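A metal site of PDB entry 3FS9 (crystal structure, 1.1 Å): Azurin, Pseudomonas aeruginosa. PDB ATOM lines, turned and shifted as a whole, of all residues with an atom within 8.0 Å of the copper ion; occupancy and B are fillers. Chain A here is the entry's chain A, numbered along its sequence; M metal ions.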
ATOM      1  N   GLY A   9     -14.549 -28.225 -30.486  1.00  0.00           N
ATOM      2  CA  GLY A   9     -14.576 -28.829 -29.146  1.00  0.00           C
ATOM      3  C   GLY A   9     -14.924 -30.297 -29.309  1.00  0.00           C
ATOM      4  O   GLY A   9     -15.858 -30.615 -30.052  1.00  0.00           O
ATOM      5  N   ASN A  10     -14.186 -31.174 -28.640  1.00  0.00           N
ATOM      6  CA  ASN A  10     -14.298 -32.606 -28.915  1.00  0.00           C
ATOM      7  C   ASN A  10     -14.786 -33.453 -27.758  1.00  0.00           C
ATOM      8  O   ASN A  10     -15.231 -32.923 -26.708  1.00  0.00           O
ATOM      9  CB  ASN A  10     -12.963 -33.105 -29.457  1.00  0.00           C
ATOM     10  CG  ASN A  10     -11.907 -33.188 -28.382  1.00  0.00           C
ATOM     11  OD1 ASN A  10     -12.150 -32.994 -27.194  1.00  0.00           O
ATOM     12  ND2 ASN A  10     -10.707 -33.673 -28.825  1.00  0.00           N
ATOM     13  N   MET A  13     -13.333 -33.139 -24.004  1.00  0.00           N
ATOM     14  CA  MET A  13     -13.480 -31.923 -23.221  1.00  0.00           C
ATOM     15  C   MET A  13     -12.320 -30.956 -23.472  1.00  0.00           C
ATOM     16  O   MET A  13     -11.772 -30.361 -22.541  1.00  0.00           O
ATOM     17  CB  MET A  13     -13.686 -32.240 -21.718  1.00  0.00           C
ATOM     18  CG  MET A  13     -14.275 -31.033 -20.946  1.00  0.00           C
ATOM     19  SD  MET A  13     -14.213 -31.290 -19.191  1.00  0.00           S
ATOM     20  CE  MET A  13     -12.459 -30.994 -18.917  1.00  0.00           C
ATOM     21  N   GLN A  14     -12.006 -30.746 -24.746  1.00  0.00           N
ATOM     22  CA  GLN A  14     -11.080 -29.694 -25.053  1.00  0.00           C
ATOM     23  C   GLN A  14     -11.350 -29.045 -26.418  1.00  0.00           C
ATOM     24  O   GLN A  14     -11.900 -29.615 -27.383  1.00  0.00           O
ATOM     25  CB  GLN A  14      -9.648 -30.201 -24.955  1.00  0.00           C
ATOM     26  CG  GLN A  14      -9.356 -31.247 -26.012  1.00  0.00           C
ATOM     27  CD  GLN A  14      -8.036 -31.899 -25.713  1.00  0.00           C
ATOM     28  OE1 GLN A  14      -7.796 -32.367 -24.605  1.00  0.00           O
ATOM     29  NE2 GLN A  14      -7.143 -31.845 -26.667  1.00  0.00           N
ATOM     30  N   PHE A  15     -11.018 -27.747 -26.444  1.00  0.00           N
ATOM     31  CA  PHE A  15     -10.968 -26.995 -27.689  1.00  0.00           C
ATOM     32  C   PHE A  15      -9.659 -27.333 -28.373  1.00  0.00           C
ATOM     33  O   PHE A  15      -8.685 -27.792 -27.743  1.00  0.00           O
ATOM     34  CB  PHE A  15     -10.985 -25.475 -27.448  1.00  0.00           C
ATOM     35  CG  PHE A  15     -12.298 -24.913 -26.938  1.00  0.00           C
ATOM     36  CD1 PHE A  15     -13.483 -25.034 -27.647  1.00  0.00           C
ATOM     37  CD2 PHE A  15     -12.317 -24.179 -25.776  1.00  0.00           C
ATOM     38  CE1 PHE A  15     -14.635 -24.427 -27.197  1.00  0.00           C
ATOM     39  CE2 PHE A  15     -13.482 -23.569 -25.322  1.00  0.00           C
ATOM     40  CZ  PHE A  15     -14.646 -23.712 -26.046  1.00  0.00           C
ATOM     41  N   LEU A  33     -17.792 -22.497 -34.498  1.00  0.00           N
ATOM     42  CA  LEU A  33     -17.574 -23.631 -33.588  1.00  0.00           C
ATOM     43  C   LEU A  33     -18.159 -24.901 -34.191  1.00  0.00           C
ATOM     44  O   LEU A  33     -19.291 -24.938 -34.693  1.00  0.00           O
ATOM     45  CB  LEU A  33     -18.278 -23.330 -32.279  1.00  0.00           C
ATOM     46  CG  LEU A  33     -18.072 -24.406 -31.183  1.00  0.00           C
ATOM     47  CD1 LEU A  33     -16.624 -24.506 -30.665  1.00  0.00           C
ATOM     48  CD2 LEU A  33     -19.026 -24.152 -30.008  1.00  0.00           C
ATOM     49  N   HIS A  35     -18.058 -29.535 -33.589  1.00  0.00           N
ATOM     50  CA  HIS A  35     -17.890 -30.602 -32.587  1.00  0.00           C
ATOM     51  C   HIS A  35     -17.602 -31.901 -33.330  1.00  0.00           C
ATOM     52  O   HIS A  35     -18.497 -32.668 -33.638  1.00  0.00           O
ATOM     53  CB  HIS A  35     -19.122 -30.691 -31.722  1.00  0.00           C
ATOM     54  CG  HIS A  35     -18.991 -31.621 -30.534  1.00  0.00           C
ATOM     55  ND1 HIS A  35     -18.287 -32.813 -30.527  1.00  0.00           N
ATOM     56  CD2 HIS A  35     -19.476 -31.450 -29.297  1.00  0.00           C
ATOM     57  CE1 HIS A  35     -18.417 -33.363 -29.318  1.00  0.00           C
ATOM     58  NE2 HIS A  35     -19.122 -32.556 -28.553  1.00  0.00           N
ATOM     59  N   MET A  44     -21.680 -34.439 -23.734  1.00  0.00           N
ATOM     60  CA  MET A  44     -20.459 -33.641 -23.905  1.00  0.00           C
ATOM     61  C   MET A  44     -20.720 -32.503 -24.897  1.00  0.00           C
ATOM     62  O   MET A  44     -20.054 -32.405 -25.927  1.00  0.00           O
ATOM     63  CB  MET A  44     -19.301 -34.576 -24.340  1.00  0.00           C
ATOM     64  CG  MET A  44     -17.933 -33.926 -24.352  1.00  0.00           C
ATOM     65  SD  MET A  44     -17.363 -33.208 -22.791  1.00  0.00           S
ATOM     66  CE  MET A  44     -17.148 -34.713 -21.828  1.00  0.00           C
ATOM     67  N   GLY A  45     -21.678 -31.668 -24.615  1.00  0.00           N
ATOM     68  CA  GLY A  45     -21.976 -30.487 -25.413  1.00  0.00           C
ATOM     69  C   GLY A  45     -21.008 -29.362 -25.050  1.00  0.00           C
ATOM     70  O   GLY A  45     -20.587 -29.254 -23.885  1.00  0.00           O
ATOM     71  N   HIS A  46     -20.691 -28.518 -26.024  1.00  0.00           N
ATOM     72  CA  HIS A  46     -19.800 -27.356 -25.820  1.00  0.00           C
ATOM     73  C   HIS A  46     -20.470 -26.099 -26.332  1.00  0.00           C
ATOM     74  O   HIS A  46     -21.236 -26.129 -27.312  1.00  0.00           O
ATOM     75  CB  HIS A  46     -18.459 -27.521 -26.517  1.00  0.00           C
ATOM     76  CG  HIS A  46     -17.738 -28.738 -26.106  1.00  0.00           C
ATOM     77  ND1 HIS A  46     -17.347 -28.967 -24.790  1.00  0.00           N
ATOM     78  CD2 HIS A  46     -17.331 -29.774 -26.873  1.00  0.00           C
ATOM     79  CE1 HIS A  46     -16.706 -30.113 -24.811  1.00  0.00           C
ATOM     80  NE2 HIS A  46     -16.686 -30.628 -26.034  1.00  0.00           N
ATOM     81  N   ASN A  47     -20.111 -24.979 -25.735  1.00  0.00           N
ATOM     82  CA  ASN A  47     -20.339 -23.674 -26.386  1.00  0.00           C
ATOM     83  C   ASN A  47     -19.019 -22.862 -26.305  1.00  0.00           C
ATOM     84  O   ASN A  47     -17.968 -23.373 -25.880  1.00  0.00           O
ATOM     85  CB  ASN A  47     -21.551 -22.965 -25.771  1.00  0.00           C
ATOM     86  CG  ASN A  47     -21.338 -22.503 -24.328  1.00  0.00           C
ATOM     87  OD1 ASN A  47     -20.303 -22.671 -23.771  1.00  0.00           O
ATOM     88  ND2 ASN A  47     -22.382 -21.974 -23.703  1.00  0.00           N
ATOM     89  N   TRP A  48     -19.093 -21.653 -26.792  1.00  0.00           N
ATOM     90  CA  TRP A  48     -17.950 -20.739 -26.826  1.00  0.00           C
ATOM     91  C   TRP A  48     -18.454 -19.409 -26.338  1.00  0.00           C
ATOM     92  O   TRP A  48     -19.462 -18.876 -26.850  1.00  0.00           O
ATOM     93  CB  TRP A  48     -17.416 -20.663 -28.255  1.00  0.00           C
ATOM     94  CG  TRP A  48     -16.194 -19.820 -28.409  1.00  0.00           C
ATOM     95  CD1 TRP A  48     -14.873 -20.243 -28.443  1.00  0.00           C
ATOM     96  CD2 TRP A  48     -16.121 -18.402 -28.643  1.00  0.00           C
ATOM     97  NE1 TRP A  48     -14.020 -19.207 -28.666  1.00  0.00           N
ATOM     98  CE2 TRP A  48     -14.744 -18.054 -28.768  1.00  0.00           C
ATOM     99  CE3 TRP A  48     -17.101 -17.371 -28.746  1.00  0.00           C
ATOM    100  CZ2 TRP A  48     -14.340 -16.731 -28.973  1.00  0.00           C
ATOM    101  CZ3 TRP A  48     -16.669 -16.074 -28.988  1.00  0.00           C
ATOM    102  CH2 TRP A  48     -15.324 -15.762 -29.059  1.00  0.00           C
ATOM    103  N   LEU A  86     -25.066 -24.179 -27.348  1.00  0.00           N
ATOM    104  CA  LEU A  86     -24.486 -25.467 -26.975  1.00  0.00           C
ATOM    105  C   LEU A  86     -24.688 -26.443 -28.118  1.00  0.00           C
ATOM    106  O   LEU A  86     -25.814 -26.618 -28.610  1.00  0.00           O
ATOM    107  CB  LEU A  86     -25.242 -26.037 -25.755  1.00  0.00           C
ATOM    108  CG  LEU A  86     -24.652 -27.306 -25.137  1.00  0.00           C
ATOM    109  CD1 LEU A  86     -23.477 -26.943 -24.289  1.00  0.00           C
ATOM    110  CD2 LEU A  86     -25.725 -28.080 -24.332  1.00  0.00           C
ATOM    111  N   ILE A  87     -23.597 -27.078 -28.548  1.00  0.00           N
ATOM    112  CA  ILE A  87     -23.623 -28.055 -29.647  1.00  0.00           C
ATOM    113  C   ILE A  87     -23.059 -29.395 -29.202  1.00  0.00           C
ATOM    114  O   ILE A  87     -22.153 -29.489 -28.376  1.00  0.00           O
ATOM    115  CB  ILE A  87     -22.830 -27.532 -30.883  1.00  0.00           C
ATOM    116  CG1 ILE A  87     -21.340 -27.313 -30.622  1.00  0.00           C
ATOM    117  CG2 ILE A  87     -23.513 -26.269 -31.423  1.00  0.00           C
ATOM    118  CD1 ILE A  87     -20.563 -27.068 -31.883  1.00  0.00           C
ATOM    119  N   PHE A 111     -14.068 -19.351 -23.346  1.00  0.00           N
ATOM    120  CA  PHE A 111     -14.207 -20.564 -22.547  1.00  0.00           C
ATOM    121  C   PHE A 111     -15.515 -21.235 -22.946  1.00  0.00           C
ATOM    122  O   PHE A 111     -16.402 -20.652 -23.590  1.00  0.00           O
ATOM    123  CB  PHE A 111     -14.102 -20.313 -21.056  1.00  0.00           C
ATOM    124  CG  PHE A 111     -15.092 -19.271 -20.542  1.00  0.00           C
ATOM    125  CD1 PHE A 111     -16.309 -19.654 -19.969  1.00  0.00           C
ATOM    126  CD2 PHE A 111     -14.774 -17.928 -20.631  1.00  0.00           C
ATOM    127  CE1 PHE A 111     -17.179 -18.688 -19.504  1.00  0.00           C
ATOM    128  CE2 PHE A 111     -15.687 -16.965 -20.152  1.00  0.00           C
ATOM    129  CZ  PHE A 111     -16.851 -17.372 -19.614  1.00  0.00           C
ATOM    130  N   CYS A 112     -15.674 -22.499 -22.524  1.00  0.00           N
ATOM    131  CA  CYS A 112     -16.927 -23.223 -22.600  1.00  0.00           C
ATOM    132  C   CYS A 112     -17.671 -23.078 -21.267  1.00  0.00           C
ATOM    133  O   CYS A 112     -17.090 -23.310 -20.202  1.00  0.00           O
ATOM    134  CB  CYS A 112     -16.631 -24.734 -22.879  1.00  0.00           C
ATOM    135  SG  CYS A 112     -18.149 -25.708 -22.901  1.00  0.00           S
ATOM    136  N   ALA A 113     -18.904 -22.642 -21.311  1.00  0.00           N
ATOM    137  CA  ALA A 113     -19.642 -22.425 -20.080  1.00  0.00           C
ATOM    138  C   ALA A 113     -19.900 -23.741 -19.354  1.00  0.00           C
ATOM    139  O   ALA A 113     -20.021 -23.709 -18.145  1.00  0.00           O
ATOM    140  CB  ALA A 113     -20.992 -21.783 -20.338  1.00  0.00           C
ATOM    141  N   ALA A 114     -20.104 -24.847 -20.089  1.00  0.00           N
ATOM    142  CA  ALA A 114     -20.365 -26.172 -19.539  1.00  0.00           C
ATOM    143  C   ALA A 114     -19.101 -26.695 -18.829  1.00  0.00           C
ATOM    144  O   ALA A 114     -19.148 -27.380 -17.778  1.00  0.00           O
ATOM    145  CB  ALA A 114     -20.825 -27.204 -20.636  1.00  0.00           C
ATOM    146  N   HIS A 115     -17.947 -26.396 -19.419  1.00  0.00           N
ATOM    147  CA  HIS A 115     -16.648 -26.918 -19.010  1.00  0.00           C
ATOM    148  C   HIS A 115     -15.659 -25.779 -18.926  1.00  0.00           C
ATOM    149  O   HIS A 115     -14.887 -25.553 -19.871  1.00  0.00           O
ATOM    150  CB  HIS A 115     -16.166 -27.943 -20.049  1.00  0.00           C
ATOM    151  CG  HIS A 115     -17.165 -28.971 -20.390  1.00  0.00           C
ATOM    152  ND1 HIS A 115     -17.644 -29.105 -21.672  1.00  0.00           N
ATOM    153  CD2 HIS A 115     -17.757 -29.928 -19.643  1.00  0.00           C
ATOM    154  CE1 HIS A 115     -18.516 -30.109 -21.665  1.00  0.00           C
ATOM    155  NE2 HIS A 115     -18.598 -30.631 -20.441  1.00  0.00           N
ATOM    156  N   ALA A 116     -15.657 -25.075 -17.829  1.00  0.00           N
ATOM    157  CA  ALA A 116     -14.851 -23.853 -17.690  1.00  0.00           C
ATOM    158  C   ALA A 116     -13.393 -24.135 -17.712  1.00  0.00           C
ATOM    159  O   ALA A 116     -12.589 -23.189 -17.924  1.00  0.00           O
ATOM    160  CB  ALA A 116     -15.267 -23.089 -16.439  1.00  0.00           C
ATOM    161  N   ALA A 117     -12.969 -25.373 -17.528  1.00  0.00           N
ATOM    162  CA  ALA A 117     -11.575 -25.735 -17.744  1.00  0.00           C
ATOM    163  C   ALA A 117     -11.114 -25.527 -19.174  1.00  0.00           C
ATOM    164  O   ALA A 117      -9.904 -25.411 -19.430  1.00  0.00           O
ATOM    165  CB  ALA A 117     -11.336 -27.190 -17.313  1.00  0.00           C
ATOM    166  N   MET A 118     -12.068 -25.580 -20.131  1.00  0.00           N
ATOM    167  CA  MET A 118     -11.814 -25.345 -21.577  1.00  0.00           C
ATOM    168  C   MET A 118     -11.750 -23.852 -21.804  1.00  0.00           C
ATOM    169  O   MET A 118     -12.765 -23.177 -21.701  1.00  0.00           O
ATOM    170  CB  MET A 118     -12.926 -25.914 -22.446  1.00  0.00           C
ATOM    171  CG  MET A 118     -13.079 -27.413 -22.380  1.00  0.00           C
ATOM    172  SD  MET A 118     -14.497 -28.073 -23.270  1.00  0.00           S
ATOM    173  CE  MET A 118     -14.250 -27.400 -24.928  1.00  0.00           C
HETATM  174 CU    CU M   1     -17.499 -27.778 -23.190  1.00  0.00          CU
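The copper ion is bound by ND1 of His 46, ND1 of His 115 and SG of Cys 112.
Slightly farther from the copper ion lies the side-chain sulfur (SD) of Met 118 (3.0 Å).
O of Gly 45 touches the copper ion (3.5 Å).
Of the 22 residues printed, 5 come within 4 Å of the copper ion.
Along chain A the residues within 4 Å of the copper ion span positions 45 to 118.
The nearest printed residue that does not touch the copper ion is Ala 114 (4.2 Å).
The side-chain sulfur (SD) of Met 118 sits close to a ring nitrogen (ND1) of His 46, at 3.4 Å.
SG of Cys 112 lies close to N of Asn 47 (3.5 Å).
O of Asn 10 lies within hydrogen-bond range of NE2 of His 46 (2.8 Å).
NE2 of His 115 lies close to SD of Met 44, at 3.7 Å.
N of Cys 112 sits at hydrogen-bond distance from O of Met 118, at 3.1 Å.
The backbone carbonyl oxygen (O) of His 46 sits at hydrogen-bond distance from the backbone NH (N) of Ile 87, at 2.8 Å.
The side-chain sulfur (SG) of Cys 112 lies close to the backbone NH (N) of Ala 114 (3.5 Å).
The side-chain sulfur (SD) of Met 118 sits close to a ring nitrogen (ND1) of His 115.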
